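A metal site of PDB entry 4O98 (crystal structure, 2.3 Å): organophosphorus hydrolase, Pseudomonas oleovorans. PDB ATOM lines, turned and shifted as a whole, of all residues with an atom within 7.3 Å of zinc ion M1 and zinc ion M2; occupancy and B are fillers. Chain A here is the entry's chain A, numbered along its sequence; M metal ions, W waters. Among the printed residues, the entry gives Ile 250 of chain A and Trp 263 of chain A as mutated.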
ATOM      1  N   ALA A  88      23.325 -14.866   6.631  1.00  0.00           N
ATOM      2  CA  ALA A  88      22.022 -14.871   5.951  1.00  0.00           C
ATOM      3  C   ALA A  88      22.135 -15.422   4.528  1.00  0.00           C
ATOM      4  O   ALA A  88      23.200 -15.354   3.904  1.00  0.00           O
ATOM      5  CB  ALA A  88      21.408 -13.461   5.913  1.00  0.00           C
ATOM      6  N   VAL A  89      21.030 -15.996   4.036  1.00  0.00           N
ATOM      7  CA  VAL A  89      20.887 -16.416   2.651  1.00  0.00           C
ATOM      8  C   VAL A  89      19.637 -15.717   2.125  1.00  0.00           C
ATOM      9  O   VAL A  89      18.551 -15.903   2.684  1.00  0.00           O
ATOM     10  CB  VAL A  89      20.739 -17.933   2.535  1.00  0.00           C
ATOM     11  CG1 VAL A  89      20.484 -18.345   1.076  1.00  0.00           C
ATOM     12  CG2 VAL A  89      21.978 -18.642   3.077  1.00  0.00           C
ATOM     13  N   ASP A 104      17.656 -15.933  -7.682  1.00  0.00           N
ATOM     14  CA  ASP A 104      18.033 -16.964  -6.697  1.00  0.00           C
ATOM     15  C   ASP A 104      16.819 -17.441  -5.905  1.00  0.00           C
ATOM     16  O   ASP A 104      15.726 -16.841  -5.981  1.00  0.00           O
ATOM     17  CB  ASP A 104      19.192 -16.528  -5.785  1.00  0.00           C
ATOM     18  CG  ASP A 104      20.488 -16.291  -6.559  1.00  0.00           C
ATOM     19  OD1 ASP A 104      20.660 -16.860  -7.648  1.00  0.00           O
ATOM     20  OD2 ASP A 104      21.352 -15.537  -6.068  1.00  0.00           O
ATOM     21  N   PHE A 111      20.789 -27.692   2.689  1.00  0.00           N
ATOM     22  CA  PHE A 111      21.761 -27.295   3.707  1.00  0.00           C
ATOM     23  C   PHE A 111      21.184 -27.401   5.119  1.00  0.00           C
ATOM     24  O   PHE A 111      21.633 -26.707   6.029  1.00  0.00           O
ATOM     25  CB  PHE A 111      22.279 -25.870   3.476  1.00  0.00           C
ATOM     26  CG  PHE A 111      23.383 -25.772   2.453  1.00  0.00           C
ATOM     27  CD1 PHE A 111      23.901 -26.905   1.860  1.00  0.00           C
ATOM     28  CD2 PHE A 111      23.922 -24.548   2.112  1.00  0.00           C
ATOM     29  CE1 PHE A 111      24.931 -26.823   0.924  1.00  0.00           C
ATOM     30  CE2 PHE A 111      24.952 -24.448   1.189  1.00  0.00           C
ATOM     31  CZ  PHE A 111      25.457 -25.586   0.595  1.00  0.00           C
ATOM     32  N   THR A 138      22.233 -16.439 -10.046  1.00  0.00           N
ATOM     33  CA  THR A 138      23.559 -15.821 -10.041  1.00  0.00           C
ATOM     34  C   THR A 138      24.618 -16.894 -10.272  1.00  0.00           C
ATOM     35  O   THR A 138      25.623 -16.639 -10.947  1.00  0.00           O
ATOM     36  CB  THR A 138      23.857 -15.021  -8.743  1.00  0.00           C
ATOM     37  OG1 THR A 138      23.606 -15.853  -7.592  1.00  0.00           O
ATOM     38  CG2 THR A 138      22.975 -13.775  -8.669  1.00  0.00           C
ATOM     39  N   HIS A 139      24.371 -18.078  -9.713  1.00  0.00           N
ATOM     40  CA  HIS A 139      25.245 -19.253  -9.859  1.00  0.00           C
ATOM     41  C   HIS A 139      24.534 -20.476  -9.276  1.00  0.00           C
ATOM     42  O   HIS A 139      23.477 -20.343  -8.643  1.00  0.00           O
ATOM     43  CB  HIS A 139      26.613 -19.037  -9.184  1.00  0.00           C
ATOM     44  CG  HIS A 139      26.555 -18.781  -7.705  1.00  0.00           C
ATOM     45  ND1 HIS A 139      25.808 -17.758  -7.157  1.00  0.00           N
ATOM     46  CD2 HIS A 139      27.173 -19.395  -6.672  1.00  0.00           C
ATOM     47  CE1 HIS A 139      25.969 -17.758  -5.842  1.00  0.00           C
ATOM     48  NE2 HIS A 139      26.785 -18.742  -5.516  1.00  0.00           N
ATOM     49  N   LEU A 140      25.107 -21.665  -9.489  1.00  0.00           N
ATOM     50  CA  LEU A 140      24.403 -22.927  -9.196  1.00  0.00           C
ATOM     51  C   LEU A 140      24.715 -23.572  -7.841  1.00  0.00           C
ATOM     52  O   LEU A 140      24.414 -24.749  -7.632  1.00  0.00           O
ATOM     53  CB  LEU A 140      24.616 -23.961 -10.319  1.00  0.00           C
ATOM     54  CG  LEU A 140      23.808 -23.775 -11.599  1.00  0.00           C
ATOM     55  CD1 LEU A 140      24.359 -24.669 -12.688  1.00  0.00           C
ATOM     56  CD2 LEU A 140      22.331 -24.063 -11.357  1.00  0.00           C
ATOM     57  N   HIS A 141      25.327 -22.811  -6.927  1.00  0.00           N
ATOM     58  CA  HIS A 141      25.525 -23.297  -5.561  1.00  0.00           C
ATOM     59  C   HIS A 141      24.182 -23.673  -4.931  1.00  0.00           C
ATOM     60  O   HIS A 141      23.146 -23.104  -5.300  1.00  0.00           O
ATOM     61  CB  HIS A 141      26.238 -22.231  -4.726  1.00  0.00           C
ATOM     62  CG  HIS A 141      27.734 -22.364  -4.744  1.00  0.00           C
ATOM     63  ND1 HIS A 141      28.569 -21.342  -4.334  1.00  0.00           N
ATOM     64  CD2 HIS A 141      28.532 -23.386  -5.119  1.00  0.00           C
ATOM     65  CE1 HIS A 141      29.828 -21.735  -4.463  1.00  0.00           C
ATOM     66  NE2 HIS A 141      29.834 -22.970  -4.933  1.00  0.00           N
ATOM     67  N   PRO A 142      24.202 -24.635  -3.984  1.00  0.00           N
ATOM     68  CA  PRO A 142      22.953 -25.148  -3.423  1.00  0.00           C
ATOM     69  C   PRO A 142      22.098 -24.075  -2.767  1.00  0.00           C
ATOM     70  O   PRO A 142      20.869 -24.175  -2.853  1.00  0.00           O
ATOM     71  CB  PRO A 142      23.433 -26.142  -2.360  1.00  0.00           C
ATOM     72  CG  PRO A 142      24.786 -26.577  -2.837  1.00  0.00           C
ATOM     73  CD  PRO A 142      25.376 -25.332  -3.445  1.00  0.00           C
ATOM     74  N   ASP A 143      22.727 -23.078  -2.133  1.00  0.00           N
ATOM     75  CA  ASP A 143      21.984 -22.049  -1.404  1.00  0.00           C
ATOM     76  C   ASP A 143      21.356 -21.002  -2.326  1.00  0.00           C
ATOM     77  O   ASP A 143      20.728 -20.045  -1.847  1.00  0.00           O
ATOM     78  CB  ASP A 143      22.834 -21.360  -0.315  1.00  0.00           C
ATOM     79  CG  ASP A 143      24.174 -20.850  -0.848  1.00  0.00           C
ATOM     80  OD1 ASP A 143      24.844 -21.603  -1.589  1.00  0.00           O
ATOM     81  OD2 ASP A 143      24.565 -19.705  -0.498  1.00  0.00           O
ATOM     82  N   HIS A 144      21.508 -21.212  -3.636  1.00  0.00           N
ATOM     83  CA  HIS A 144      20.901 -20.329  -4.642  1.00  0.00           C
ATOM     84  C   HIS A 144      19.961 -21.102  -5.570  1.00  0.00           C
ATOM     85  O   HIS A 144      18.922 -20.578  -5.985  1.00  0.00           O
ATOM     86  CB  HIS A 144      21.988 -19.615  -5.438  1.00  0.00           C
ATOM     87  CG  HIS A 144      22.845 -18.731  -4.593  1.00  0.00           C
ATOM     88  ND1 HIS A 144      23.852 -19.221  -3.794  1.00  0.00           N
ATOM     89  CD2 HIS A 144      22.785 -17.398  -4.360  1.00  0.00           C
ATOM     90  CE1 HIS A 144      24.405 -18.227  -3.131  1.00  0.00           C
ATOM     91  NE2 HIS A 144      23.778 -17.104  -3.453  1.00  0.00           N
ATOM     92  N   HIS A 226      33.906 -16.706  -8.025  1.00  0.00           N
ATOM     93  CA  HIS A 226      33.312 -17.445  -6.923  1.00  0.00           C
ATOM     94  C   HIS A 226      32.830 -18.783  -7.456  1.00  0.00           C
ATOM     95  O   HIS A 226      33.051 -19.815  -6.809  1.00  0.00           O
ATOM     96  CB  HIS A 226      32.183 -16.642  -6.285  1.00  0.00           C
ATOM     97  CG  HIS A 226      31.411 -17.404  -5.243  1.00  0.00           C
ATOM     98  ND1 HIS A 226      31.934 -17.673  -3.994  1.00  0.00           N
ATOM     99  CD2 HIS A 226      30.183 -17.954  -5.275  1.00  0.00           C
ATOM    100  CE1 HIS A 226      31.048 -18.365  -3.299  1.00  0.00           C
ATOM    101  NE2 HIS A 226      29.968 -18.551  -4.055  1.00  0.00           N
ATOM    102  N   THR A 227      32.186 -18.764  -8.619  1.00  0.00           N
ATOM    103  CA  THR A 227      32.039 -19.967  -9.458  1.00  0.00           C
ATOM    104  C   THR A 227      32.423 -19.570 -10.892  1.00  0.00           C
ATOM    105  O   THR A 227      32.534 -18.360 -11.190  1.00  0.00           O
ATOM    106  CB  THR A 227      30.601 -20.529  -9.458  1.00  0.00           C
ATOM    107  OG1 THR A 227      29.732 -19.568 -10.064  1.00  0.00           O
ATOM    108  CG2 THR A 227      30.118 -20.839  -8.047  1.00  0.00           C
ATOM    109  N   HIS A 230      29.644 -17.301 -12.361  1.00  0.00           N
ATOM    110  CA  HIS A 230      28.931 -16.441 -11.418  1.00  0.00           C
ATOM    111  C   HIS A 230      28.575 -15.126 -12.089  1.00  0.00           C
ATOM    112  O   HIS A 230      29.425 -14.486 -12.725  1.00  0.00           O
ATOM    113  CB  HIS A 230      29.790 -16.176 -10.178  1.00  0.00           C
ATOM    114  CG  HIS A 230      29.079 -15.397  -9.111  1.00  0.00           C
ATOM    115  ND1 HIS A 230      29.056 -14.017  -9.079  1.00  0.00           N
ATOM    116  CD2 HIS A 230      28.330 -15.818  -8.061  1.00  0.00           C
ATOM    117  CE1 HIS A 230      28.345 -13.615  -8.041  1.00  0.00           C
ATOM    118  NE2 HIS A 230      27.894 -14.691  -7.402  1.00  0.00           N
ATOM    119  N   GLY A 246      24.665 -11.441  -6.087  1.00  0.00           N
ATOM    120  CA  GLY A 246      25.021 -12.815  -5.733  1.00  0.00           C
ATOM    121  C   GLY A 246      26.067 -12.885  -4.628  1.00  0.00           C
ATOM    122  O   GLY A 246      25.915 -12.265  -3.566  1.00  0.00           O
ATOM    123  N   ASP A 247      27.119 -13.658  -4.868  1.00  0.00           N
ATOM    124  CA  ASP A 247      28.103 -13.955  -3.845  1.00  0.00           C
ATOM    125  C   ASP A 247      29.443 -13.244  -4.079  1.00  0.00           C
ATOM    126  O   ASP A 247      30.507 -13.806  -3.876  1.00  0.00           O
ATOM    127  CB  ASP A 247      28.313 -15.469  -3.737  1.00  0.00           C
ATOM    128  CG  ASP A 247      27.181 -16.161  -2.979  1.00  0.00           C
ATOM    129  OD1 ASP A 247      26.085 -15.558  -2.863  1.00  0.00           O
ATOM    130  OD2 ASP A 247      27.382 -17.299  -2.503  1.00  0.00           O
ATOM    131  N   LEU A 249      30.630 -11.366  -2.208  1.00  0.00           N
ATOM    132  CA  LEU A 249      31.157 -11.177  -0.882  1.00  0.00           C
ATOM    133  C   LEU A 249      30.336 -12.056   0.061  1.00  0.00           C
ATOM    134  O   LEU A 249      29.126 -12.172  -0.119  1.00  0.00           O
ATOM    135  CB  LEU A 249      30.970  -9.701  -0.556  1.00  0.00           C
ATOM    136  CG  LEU A 249      31.414  -9.025   0.716  1.00  0.00           C
ATOM    137  CD1 LEU A 249      31.624  -7.548   0.363  1.00  0.00           C
ATOM    138  CD2 LEU A 249      30.337  -9.217   1.758  1.00  0.00           C
ATOM    139  N   ILE A 250      30.992 -12.698   1.025  1.00  0.00           N
ATOM    140  CA  ILE A 250      30.277 -13.611   1.922  1.00  0.00           C
ATOM    141  C   ILE A 250      30.149 -13.084   3.356  1.00  0.00           C
ATOM    142  O   ILE A 250      29.190 -13.402   4.060  1.00  0.00           O
ATOM    143  CB  ILE A 250      30.919 -15.016   1.953  1.00  0.00           C
ATOM    144  CG1 ILE A 250      31.254 -15.515   0.549  1.00  0.00           C
ATOM    145  CG2 ILE A 250      29.990 -16.021   2.675  1.00  0.00           C
ATOM    146  CD1 ILE A 250      30.040 -16.084  -0.234  1.00  0.00           C
ATOM    147  N   TRP A 263      37.357 -16.429   0.230  1.00  0.00           N
ATOM    148  CA  TRP A 263      36.522 -17.447   0.854  1.00  0.00           C
ATOM    149  C   TRP A 263      36.959 -18.821   0.366  1.00  0.00           C
ATOM    150  O   TRP A 263      37.184 -19.016  -0.847  1.00  0.00           O
ATOM    151  CB  TRP A 263      35.071 -17.177   0.444  1.00  0.00           C
ATOM    152  CG  TRP A 263      34.075 -18.052   1.089  1.00  0.00           C
ATOM    153  CD1 TRP A 263      33.302 -19.012   0.487  1.00  0.00           C
ATOM    154  CD2 TRP A 263      33.704 -18.036   2.460  1.00  0.00           C
ATOM    155  NE1 TRP A 263      32.477 -19.596   1.412  1.00  0.00           N
ATOM    156  CE2 TRP A 263      32.714 -19.022   2.628  1.00  0.00           C
ATOM    157  CE3 TRP A 263      34.116 -17.290   3.569  1.00  0.00           C
ATOM    158  CZ2 TRP A 263      32.116 -19.269   3.869  1.00  0.00           C
ATOM    159  CZ3 TRP A 263      33.533 -17.532   4.786  1.00  0.00           C
ATOM    160  CH2 TRP A 263      32.543 -18.518   4.930  1.00  0.00           C
ATOM    161  N   PHE A 265      35.478 -21.504  -0.298  1.00  0.00           N
ATOM    162  CA  PHE A 265      34.675 -22.126  -1.344  1.00  0.00           C
ATOM    163  C   PHE A 265      34.471 -21.293  -2.616  1.00  0.00           C
ATOM    164  O   PHE A 265      33.595 -21.611  -3.424  1.00  0.00           O
ATOM    165  CB  PHE A 265      33.332 -22.607  -0.806  1.00  0.00           C
ATOM    166  CG  PHE A 265      33.461 -23.689   0.212  1.00  0.00           C
ATOM    167  CD1 PHE A 265      33.642 -23.385   1.559  1.00  0.00           C
ATOM    168  CD2 PHE A 265      33.432 -25.024  -0.168  1.00  0.00           C
ATOM    169  CE1 PHE A 265      33.785 -24.393   2.510  1.00  0.00           C
ATOM    170  CE2 PHE A 265      33.569 -26.035   0.771  1.00  0.00           C
ATOM    171  CZ  PHE A 265      33.754 -25.722   2.114  1.00  0.00           C
ATOM    172  N   ASP A 266      35.258 -20.229  -2.771  1.00  0.00           N
ATOM    173  CA  ASP A 266      35.409 -19.631  -4.095  1.00  0.00           C
ATOM    174  C   ASP A 266      36.136 -20.658  -4.976  1.00  0.00           C
ATOM    175  O   ASP A 266      37.252 -21.072  -4.657  1.00  0.00           O
ATOM    176  CB  ASP A 266      36.265 -18.358  -4.034  1.00  0.00           C
ATOM    177  CG  ASP A 266      35.546 -17.184  -3.366  1.00  0.00           C
ATOM    178  OD1 ASP A 266      34.316 -17.048  -3.540  1.00  0.00           O
ATOM    179  OD2 ASP A 266      36.237 -16.379  -2.689  1.00  0.00           O
ATOM    180  N   ALA A 293      23.220 -11.527  -1.560  1.00  0.00           N
ATOM    181  CA  ALA A 293      22.666 -12.790  -1.077  1.00  0.00           C
ATOM    182  C   ALA A 293      23.087 -13.154   0.350  1.00  0.00           C
ATOM    183  O   ALA A 293      22.349 -13.839   1.060  1.00  0.00           O
ATOM    184  CB  ALA A 293      23.031 -13.910  -2.028  1.00  0.00           C
ATOM    185  N   HIS A 294      24.270 -12.735   0.769  1.00  0.00           N
ATOM    186  CA  HIS A 294      24.756 -13.099   2.093  1.00  0.00           C
ATOM    187  C   HIS A 294      25.019 -11.865   2.958  1.00  0.00           C
ATOM    188  O   HIS A 294      25.710 -11.951   3.982  1.00  0.00           O
ATOM    189  CB  HIS A 294      26.008 -13.995   1.977  1.00  0.00           C
ATOM    190  CG  HIS A 294      25.765 -15.279   1.246  1.00  0.00           C
ATOM    191  ND1 HIS A 294      24.812 -16.197   1.663  1.00  0.00           N
ATOM    192  CD2 HIS A 294      26.317 -15.790   0.121  1.00  0.00           C
ATOM    193  CE1 HIS A 294      24.810 -17.222   0.825  1.00  0.00           C
ATOM    194  NE2 HIS A 294      25.713 -17.004  -0.113  1.00  0.00           N
HETATM  195 ZN    ZN M   1      27.981 -19.317  -3.633  1.00  0.00          ZN
HETATM  196 ZN    ZN M   2      25.795 -18.282  -1.631  1.00  0.00          ZN
HETATM  197  O   HOH W   1      27.054 -20.155  -1.929  1.00  0.00           O
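The backbone carbonyl oxygen of Ala 88 sits at hydrogen-bond distance from a ring nitrogen (ND1) of His 294 (2.9 Å).
OD1 of Asp 247 lies within hydrogen-bond range of NE2 of His 144, at 2.8 Å.
OD1 of Asp 143 sits close to ND1 of His 144 (3.4 Å).
A ring nitrogen (ND1) of His 144 sits close to a ring nitrogen (NE2) of His 139 (3.4 Å).
N of Asp 247 lies within hydrogen-bond range of NE2 of His 230, 2.8 Å away.
The side-chain carboxylate (OD1) of Asp 266 sits at hydrogen-bond distance from a ring nitrogen (ND1) of His 226 (2.5 Å).
OG1 of Thr 138 sits at hydrogen-bond distance from ND1 of His 139 (2.9 Å).
His 144 touches zinc ion M1.
Within 4 Å of zinc ion M1: His 139, His 141, His 144, His 226 and Asp 247.
Residues that only touch zinc ion M2: His 144 (2.0 Å).
Of the 23 residues printed, 4 come within 4 Å of zinc ion M2.
Zinc ion M1 is bound by water W1, a ring nitrogen (NE2) of His 226, a ring nitrogen (ND1) of His 141, a ring nitrogen (NE2) of His 139 and the side-chain carboxylate of Asp 247.
Zinc ion M2 is bound by NE2 of His 294 (2.0 Å), OD2 of Asp 247 (2.1 Å), OD2 of Asp 143 (2.2 Å) and water W1 (2.3 Å).
Zinc ion M2 has four donor atoms within binding distance.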
